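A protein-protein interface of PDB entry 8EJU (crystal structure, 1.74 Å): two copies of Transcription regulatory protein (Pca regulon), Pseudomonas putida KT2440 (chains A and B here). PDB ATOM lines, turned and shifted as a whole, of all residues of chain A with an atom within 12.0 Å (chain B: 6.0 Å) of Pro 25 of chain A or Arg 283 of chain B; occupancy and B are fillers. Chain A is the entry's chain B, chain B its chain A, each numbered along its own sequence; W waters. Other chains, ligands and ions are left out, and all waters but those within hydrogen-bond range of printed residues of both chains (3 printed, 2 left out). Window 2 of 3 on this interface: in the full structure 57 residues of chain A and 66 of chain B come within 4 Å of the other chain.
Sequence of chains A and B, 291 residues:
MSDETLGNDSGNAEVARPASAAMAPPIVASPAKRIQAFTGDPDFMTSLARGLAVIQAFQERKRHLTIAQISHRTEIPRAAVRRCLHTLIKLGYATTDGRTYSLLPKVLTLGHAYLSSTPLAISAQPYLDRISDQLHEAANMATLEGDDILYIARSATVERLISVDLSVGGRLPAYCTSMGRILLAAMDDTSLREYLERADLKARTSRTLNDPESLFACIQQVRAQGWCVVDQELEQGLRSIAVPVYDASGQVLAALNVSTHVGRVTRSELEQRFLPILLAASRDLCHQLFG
Printed residues of chain A that touch a printed residue of chain B: Ala 24, Pro 25, Pro 26 and Ile 27.
Among the printed residues, 10 pairs touch across the chains.
Among the printed residues, no Asp or Glu carboxylate lies within 4 Å of a Lys or Arg side-chain nitrogen of the other chain.
O of Ala 24 of chain A lies close to O of Gln 225 of chain B, 3.4 Å away.
The backbone carbonyl oxygen (O) of Arg 223 of chain B lies within hydrogen-bond range of the backbone NH (N) of Ile 27 of chain A (2.9 Å).
Pro 25 of chain A touches three residues of chain B.
Of the printed residues of chain B, Ile 27 of chain A touches Arg 223 and Tyr 246.
Printed residues of chain A within 4 Å of Ala 224 of chain B: Pro 26.
Printed residues of chain A within 4 Å of Gln 225 of chain B: Ala 24 (3.4 Å) and Pro 25 (3.9 Å).
Gly 226 of chain B touches just one residue of chain A: Pro 25.
Leu 279 of chain B touches one residue of chain A.
No residue of chain A comes within 4 Å of Ala 280 of chain B.
Ser 282 of chain B touches none of the printed residues of chain A.
Of chain A, only Pro 25 comes within 4 Å of Arg 283 of chain B.
No residue of chain A comes within 4 Å of Asp 284 of chain B.
No residue of chain A comes within 4 Å of Leu 285 of chain B.
The nearest printed residue of chain B that does not touch Pro 25 of chain A is Tyr 246 of chain B (5.1 Å).
The nearest residue of chain A that does not touch Arg 283 of chain B is Ala 24 of chain A (5.1 Å).
CD1 of Trp 227 of chain B touches CB of Ala 24 of chain A, 3.8 Å away.
Ala 24 of chain A touches Leu 279 of chain B.
O of Pro 25 of chain A touches O of Gln 225 of chain B, 3.9 Å away.
Pro 25 of chain A touches Gly 226 of chain B (O to CA, 3.3 Å).
CD of Pro 25 of chain A touches NH1 of Arg 283 of chain B (3.7 Å).
Arg 223 of chain B touches Pro 26 of chain A.
O of Ala 224 of chain B touches CB of Pro 26 of chain A, 3.6 Å away.
Ile 27 of chain A touches Tyr 246 of chain B (CG1 to OH, 3.5 Å).
Water W3 lies within hydrogen-bond range of the side-chain hydroxyl of Tyr 246 of chain B (2.6 Å), the backbone carbonyl oxygen of Pro 25 of chain A (2.7 Å) and the backbone carbonyl oxygen of Pro 26 of chain A (3.4 Å).
Water W1 bridges OH of Tyr 246 of chain B (2.8 Å) and N of Val 28 of chain A (3.0 Å).
Water W2 lies within hydrogen-bond range of O of Gln 225 of chain B (2.8 Å), O of Ala 24 of chain A (3.2 Å) and NE1 of Trp 227 of chain B (3.5 Å).
No position is printed for both chains.
Of the 10 pairs that touch across the chains among the printed residues, none has its exchanged pair printed and touching as well.
O of Trp 227 of chain B sits at hydrogen-bond distance from NE2 of Gln 225 of chain B (2.9 Å).
The backbone carbonyl oxygen (O) of Tyr 246 of chain B lies within hydrogen-bond range of the side-chain sulfur (SG) of Cys 286 of chain B (3.2 Å).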
ATOM      1  N   ALA A  24     -14.285  24.401 -14.799  1.00  0.00           N
ATOM      2  CA  ALA A  24     -13.032  24.346 -15.569  1.00  0.00           C
ATOM      3  C   ALA A  24     -11.993  25.328 -15.027  1.00  0.00           C
ATOM      4  O   ALA A  24     -12.340  26.408 -14.540  1.00  0.00           O
ATOM      5  CB  ALA A  24     -13.281  24.617 -17.075  1.00  0.00           C
ATOM      6  N   PRO A  25     -10.718  24.937 -15.088  1.00  0.00           N
ATOM      7  CA  PRO A  25      -9.664  25.848 -14.658  1.00  0.00           C
ATOM      8  C   PRO A  25      -9.457  26.903 -15.707  1.00  0.00           C
ATOM      9  O   PRO A  25      -9.649  26.653 -16.914  1.00  0.00           O
ATOM     10  CB  PRO A  25      -8.433  24.928 -14.544  1.00  0.00           C
ATOM     11  CG  PRO A  25      -8.720  23.824 -15.510  1.00  0.00           C
ATOM     12  CD  PRO A  25     -10.194  23.609 -15.460  1.00  0.00           C
ATOM     13  N   PRO A  26      -9.082  28.124 -15.328  1.00  0.00           N
ATOM     14  CA  PRO A  26      -8.834  29.154 -16.339  1.00  0.00           C
ATOM     15  C   PRO A  26      -7.669  28.819 -17.267  1.00  0.00           C
ATOM     16  O   PRO A  26      -6.791  28.002 -16.961  1.00  0.00           O
ATOM     17  CB  PRO A  26      -8.580  30.423 -15.508  1.00  0.00           C
ATOM     18  CG  PRO A  26      -8.174  29.930 -14.138  1.00  0.00           C
ATOM     19  CD  PRO A  26      -8.876  28.616 -13.949  1.00  0.00           C
ATOM     20  N   ILE A  27      -7.737  29.382 -18.471  1.00  0.00           N
ATOM     21  CA  ILE A  27      -6.587  29.400 -19.373  1.00  0.00           C
ATOM     22  C   ILE A  27      -5.633  30.490 -18.901  1.00  0.00           C
ATOM     23  O   ILE A  27      -6.010  31.666 -18.833  1.00  0.00           O
ATOM     24  CB  ILE A  27      -7.004  29.621 -20.832  1.00  0.00           C
ATOM     25  CG1 ILE A  27      -7.863  28.441 -21.335  1.00  0.00           C
ATOM     26  CG2 ILE A  27      -5.749  29.775 -21.766  1.00  0.00           C
ATOM     27  CD1 ILE A  27      -8.839  28.746 -22.512  1.00  0.00           C
ATOM     28  N   VAL A  28      -4.414  30.095 -18.536  1.00  0.00           N
ATOM     29  CA  VAL A  28      -3.390  31.013 -18.046  1.00  0.00           C
ATOM     30  C   VAL A  28      -2.233  31.059 -19.046  1.00  0.00           C
ATOM     31  O   VAL A  28      -2.163  30.273 -19.994  1.00  0.00           O
ATOM     32  CB  VAL A  28      -2.868  30.608 -16.658  1.00  0.00           C
ATOM     33  CG1 VAL A  28      -3.984  30.616 -15.602  1.00  0.00           C
ATOM     34  CG2 VAL A  28      -2.214  29.215 -16.765  1.00  0.00           C
ATOM     35  N   ALA A  29      -1.292  31.971 -18.798  1.00  0.00           N
ATOM     36  CA  ALA A  29      -0.122  32.148 -19.674  1.00  0.00           C
ATOM     37  C   ALA A  29       0.892  31.008 -19.518  1.00  0.00           C
ATOM     38  O   ALA A  29       1.493  30.556 -20.499  1.00  0.00           O
ATOM     39  CB  ALA A  29       0.549  33.503 -19.390  1.00  0.00           C
ATOM     40  N   ARG B 223     -10.682  33.245 -21.155  1.00  0.00           N
ATOM     41  CA  ARG B 223      -9.541  32.933 -20.307  1.00  0.00           C
ATOM     42  C   ARG B 223      -9.978  32.642 -18.881  1.00  0.00           C
ATOM     43  O   ARG B 223      -9.521  31.666 -18.274  1.00  0.00           O
ATOM     44  CB  ARG B 223      -8.533  34.083 -20.334  1.00  0.00           C
ATOM     45  CG  ARG B 223      -7.782  34.135 -21.624  1.00  0.00           C
ATOM     46  CD  ARG B 223      -6.894  35.422 -21.591  1.00  0.00           C
ATOM     47  NE  ARG B 223      -5.978  35.491 -22.724  1.00  0.00           N
ATOM     48  CZ  ARG B 223      -5.293  36.578 -23.058  1.00  0.00           C
ATOM     49  NH1 ARG B 223      -5.401  37.708 -22.371  1.00  0.00           N
ATOM     50  NH2 ARG B 223      -4.474  36.533 -24.106  1.00  0.00           N
ATOM     51  N   ALA B 224     -10.850  33.489 -18.327  1.00  0.00           N
ATOM     52  CA  ALA B 224     -11.310  33.295 -16.946  1.00  0.00           C
ATOM     53  C   ALA B 224     -12.067  31.980 -16.795  1.00  0.00           C
ATOM     54  O   ALA B 224     -12.002  31.338 -15.743  1.00  0.00           O
ATOM     55  CB  ALA B 224     -12.200  34.463 -16.525  1.00  0.00           C
ATOM     56  N   GLN B 225     -12.817  31.581 -17.834  1.00  0.00           N
ATOM     57  CA  GLN B 225     -13.686  30.398 -17.813  1.00  0.00           C
ATOM     58  C   GLN B 225     -12.953  29.082 -17.986  1.00  0.00           C
ATOM     59  O   GLN B 225     -13.303  28.082 -17.332  1.00  0.00           O
ATOM     60  CB  GLN B 225     -14.739  30.468 -18.944  1.00  0.00           C
ATOM     61  CG  GLN B 225     -15.890  31.311 -18.518  1.00  0.00           C
ATOM     62  CD  GLN B 225     -16.816  31.693 -19.625  1.00  0.00           C
ATOM     63  OE1 GLN B 225     -17.776  32.418 -19.354  1.00  0.00           O
ATOM     64  NE2 GLN B 225     -16.566  31.240 -20.866  1.00  0.00           N
ATOM     65  N   GLY B 226     -12.046  29.018 -18.952  1.00  0.00           N
ATOM     66  CA  GLY B 226     -11.469  27.780 -19.374  1.00  0.00           C
ATOM     67  C   GLY B 226     -12.261  27.086 -20.448  1.00  0.00           C
ATOM     68  O   GLY B 226     -11.993  25.926 -20.722  1.00  0.00           O
ATOM     69  N   TRP B 227     -13.278  27.747 -21.001  1.00  0.00           N
ATOM     70  CA  TRP B 227     -14.154  27.160 -22.010  1.00  0.00           C
ATOM     71  C   TRP B 227     -14.814  28.315 -22.742  1.00  0.00           C
ATOM     72  O   TRP B 227     -14.803  29.465 -22.275  1.00  0.00           O
ATOM     73  CB  TRP B 227     -15.228  26.215 -21.392  1.00  0.00           C
ATOM     74  CG  TRP B 227     -16.027  26.841 -20.269  1.00  0.00           C
ATOM     75  CD1 TRP B 227     -15.754  26.811 -18.926  1.00  0.00           C
ATOM     76  CD2 TRP B 227     -17.190  27.621 -20.421  1.00  0.00           C
ATOM     77  NE1 TRP B 227     -16.689  27.544 -18.241  1.00  0.00           N
ATOM     78  CE2 TRP B 227     -17.616  28.006 -19.133  1.00  0.00           C
ATOM     79  CE3 TRP B 227     -17.963  27.999 -21.541  1.00  0.00           C
ATOM     80  CZ2 TRP B 227     -18.719  28.805 -18.938  1.00  0.00           C
ATOM     81  CZ3 TRP B 227     -19.087  28.761 -21.333  1.00  0.00           C
ATOM     82  CH2 TRP B 227     -19.453  29.164 -20.038  1.00  0.00           C
ATOM     83  N   TYR B 246      -4.347  20.435 -23.725  1.00  0.00           N
ATOM     84  CA  TYR B 246      -3.033  20.798 -23.202  1.00  0.00           C
ATOM     85  C   TYR B 246      -2.042  19.661 -23.407  1.00  0.00           C
ATOM     86  O   TYR B 246      -2.427  18.493 -23.516  1.00  0.00           O
ATOM     87  CB  TYR B 246      -3.126  21.087 -21.700  1.00  0.00           C
ATOM     88  CG  TYR B 246      -3.860  22.330 -21.328  1.00  0.00           C
ATOM     89  CD1 TYR B 246      -3.240  23.572 -21.400  1.00  0.00           C
ATOM     90  CD2 TYR B 246      -5.168  22.267 -20.851  1.00  0.00           C
ATOM     91  CE1 TYR B 246      -3.913  24.745 -21.026  1.00  0.00           C
ATOM     92  CE2 TYR B 246      -5.844  23.447 -20.460  1.00  0.00           C
ATOM     93  CZ  TYR B 246      -5.201  24.673 -20.560  1.00  0.00           C
ATOM     94  OH  TYR B 246      -5.841  25.838 -20.189  1.00  0.00           O
ATOM     95  N   LEU B 278     -16.659  17.208 -22.304  1.00  0.00           N
ATOM     96  CA  LEU B 278     -15.503  17.725 -23.027  1.00  0.00           C
ATOM     97  C   LEU B 278     -14.293  17.871 -22.117  1.00  0.00           C
ATOM     98  O   LEU B 278     -13.158  17.522 -22.525  1.00  0.00           O
ATOM     99  CB  LEU B 278     -15.858  19.079 -23.662  1.00  0.00           C
ATOM    100  CG  LEU B 278     -16.592  19.044 -24.979  1.00  0.00           C
ATOM    101  CD1 LEU B 278     -16.999  20.396 -25.420  1.00  0.00           C
ATOM    102  CD2 LEU B 278     -15.688  18.428 -26.113  1.00  0.00           C
ATOM    103  N   LEU B 279     -14.491  18.438 -20.906  1.00  0.00           N
ATOM    104  CA  LEU B 279     -13.352  18.600 -20.007  1.00  0.00           C
ATOM    105  C   LEU B 279     -12.742  17.242 -19.666  1.00  0.00           C
ATOM    106  O   LEU B 279     -11.517  17.096 -19.605  1.00  0.00           O
ATOM    107  CB  LEU B 279     -13.751  19.348 -18.722  1.00  0.00           C
ATOM    108  CG  LEU B 279     -14.161  20.797 -18.977  1.00  0.00           C
ATOM    109  CD1 LEU B 279     -14.928  21.411 -17.777  1.00  0.00           C
ATOM    110  CD2 LEU B 279     -12.936  21.685 -19.354  1.00  0.00           C
ATOM    111  N   ALA B 280     -13.586  16.233 -19.436  1.00  0.00           N
ATOM    112  CA  ALA B 280     -13.085  14.904 -19.080  1.00  0.00           C
ATOM    113  C   ALA B 280     -12.321  14.277 -20.237  1.00  0.00           C
ATOM    114  O   ALA B 280     -11.261  13.678 -20.030  1.00  0.00           O
ATOM    115  CB  ALA B 280     -14.247  14.016 -18.634  1.00  0.00           C
ATOM    116  N   ALA B 281     -12.857  14.393 -21.468  1.00  0.00           N
ATOM    117  CA  ALA B 281     -12.189  13.849 -22.636  1.00  0.00           C
ATOM    118  C   ALA B 281     -10.838  14.510 -22.868  1.00  0.00           C
ATOM    119  O   ALA B 281      -9.847  13.843 -23.222  1.00  0.00           O
ATOM    120  CB  ALA B 281     -13.097  14.030 -23.837  1.00  0.00           C
ATOM    121  N   SER B 282     -10.813  15.829 -22.756  1.00  0.00           N
ATOM    122  CA  SER B 282      -9.565  16.540 -23.020  1.00  0.00           C
ATOM    123  C   SER B 282      -8.510  16.185 -21.978  1.00  0.00           C
ATOM    124  O   SER B 282      -7.320  16.000 -22.323  1.00  0.00           O
ATOM    125  CB  SER B 282      -9.824  18.038 -23.026  1.00  0.00           C
ATOM    126  OG  SER B 282      -8.576  18.632 -23.320  1.00  0.00           O
ATOM    127  N   ARG B 283      -8.921  16.074 -20.698  1.00  0.00           N
ATOM    128  CA  ARG B 283      -7.967  15.658 -19.670  1.00  0.00           C
ATOM    129  C   ARG B 283      -7.470  14.258 -19.944  1.00  0.00           C
ATOM    130  O   ARG B 283      -6.279  13.978 -19.749  1.00  0.00           O
ATOM    131  CB  ARG B 283      -8.547  15.733 -18.247  1.00  0.00           C
ATOM    132  CG  ARG B 283      -9.244  16.996 -17.876  1.00  0.00           C
ATOM    133  CD  ARG B 283      -9.029  17.461 -16.410  1.00  0.00           C
ATOM    134  NE  ARG B 283     -10.279  17.856 -15.754  1.00  0.00           N
ATOM    135  CZ  ARG B 283     -10.784  19.087 -15.778  1.00  0.00           C
ATOM    136  NH1 ARG B 283     -10.221  20.054 -16.484  1.00  0.00           N
ATOM    137  NH2 ARG B 283     -11.897  19.349 -15.094  1.00  0.00           N
ATOM    138  N   ASP B 284      -8.379  13.352 -20.363  1.00  0.00           N
ATOM    139  CA  ASP B 284      -7.989  11.984 -20.673  1.00  0.00           C
ATOM    140  C   ASP B 284      -6.980  11.952 -21.804  1.00  0.00           C
ATOM    141  O   ASP B 284      -6.033  11.159 -21.780  1.00  0.00           O
ATOM    142  CB  ASP B 284      -9.218  11.143 -21.062  1.00  0.00           C
ATOM    143  CG  ASP B 284     -10.048  10.719 -19.847  1.00  0.00           C
ATOM    144  OD1 ASP B 284      -9.637  10.891 -18.678  1.00  0.00           O
ATOM    145  OD2 ASP B 284     -11.182  10.237 -20.089  1.00  0.00           O
ATOM    146  N   LEU B 285      -7.216  12.767 -22.833  1.00  0.00           N
ATOM    147  CA  LEU B 285      -6.337  12.751 -23.994  1.00  0.00           C
ATOM    148  C   LEU B 285      -4.960  13.238 -23.591  1.00  0.00           C
ATOM    149  O   LEU B 285      -3.942  12.662 -24.004  1.00  0.00           O
ATOM    150  CB  LEU B 285      -6.955  13.617 -25.094  1.00  0.00           C
ATOM    151  CG  LEU B 285      -6.154  13.808 -26.378  1.00  0.00           C
ATOM    152  CD1 LEU B 285      -5.941  12.445 -26.994  1.00  0.00           C
ATOM    153  CD2 LEU B 285      -7.053  14.683 -27.231  1.00  0.00           C
ATOM    154  N   CYS B 286      -4.912  14.337 -22.845  1.00  0.00           N
ATOM    155  CA  CYS B 286      -3.632  14.871 -22.412  1.00  0.00           C
ATOM    156  C   CYS B 286      -2.863  13.823 -21.621  1.00  0.00           C
ATOM    157  O   CYS B 286      -1.681  13.544 -21.894  1.00  0.00           O
ATOM    158  CB  CYS B 286      -3.879  16.147 -21.597  1.00  0.00           C
ATOM    159  SG  CYS B 286      -2.385  16.821 -20.807  1.00  0.00           S
ATOM    160  N   HIS B 287      -3.543  13.158 -20.675  1.00  0.00           N
ATOM    161  CA  HIS B 287      -2.832  12.197 -19.840  1.00  0.00           C
ATOM    162  C   HIS B 287      -2.355  10.999 -20.651  1.00  0.00           C
ATOM    163  O   HIS B 287      -1.261  10.481 -20.414  1.00  0.00           O
ATOM    164  CB  HIS B 287      -3.728  11.734 -18.698  1.00  0.00           C
ATOM    165  CG  HIS B 287      -3.031  10.842 -17.719  1.00  0.00           C
ATOM    166  ND1 HIS B 287      -2.928   9.476 -17.889  1.00  0.00           N
ATOM    167  CD2 HIS B 287      -2.387  11.127 -16.563  1.00  0.00           C
ATOM    168  CE1 HIS B 287      -2.261   8.957 -16.871  1.00  0.00           C
ATOM    169  NE2 HIS B 287      -1.921   9.938 -16.054  1.00  0.00           N
ATOM    170  N   GLN B 288      -3.166  10.565 -21.623  1.00  0.00           N
ATOM    171  CA  GLN B 288      -2.815   9.429 -22.447  1.00  0.00           C
ATOM    172  C   GLN B 288      -1.587   9.738 -23.289  1.00  0.00           C
ATOM    173  O   GLN B 288      -0.663   8.920 -23.364  1.00  0.00           O
ATOM    174  CB  GLN B 288      -3.995   9.079 -23.343  1.00  0.00           C
ATOM    175  CG  GLN B 288      -3.788   7.922 -24.251  1.00  0.00           C
ATOM    176  CD  GLN B 288      -4.981   7.715 -25.143  1.00  0.00           C
ATOM    177  OE1 GLN B 288      -6.128   7.592 -24.673  1.00  0.00           O
ATOM    178  NE2 GLN B 288      -4.726   7.671 -26.451  1.00  0.00           N
HETATM  179  O   HOH W   1      -3.779  27.163 -18.861  1.00  0.00           O
HETATM  180  O   HOH W   2     -15.067  27.880 -15.182  1.00  0.00           O
HETATM  181  O   HOH W   3      -8.094  25.517 -18.860  1.00  0.00           O
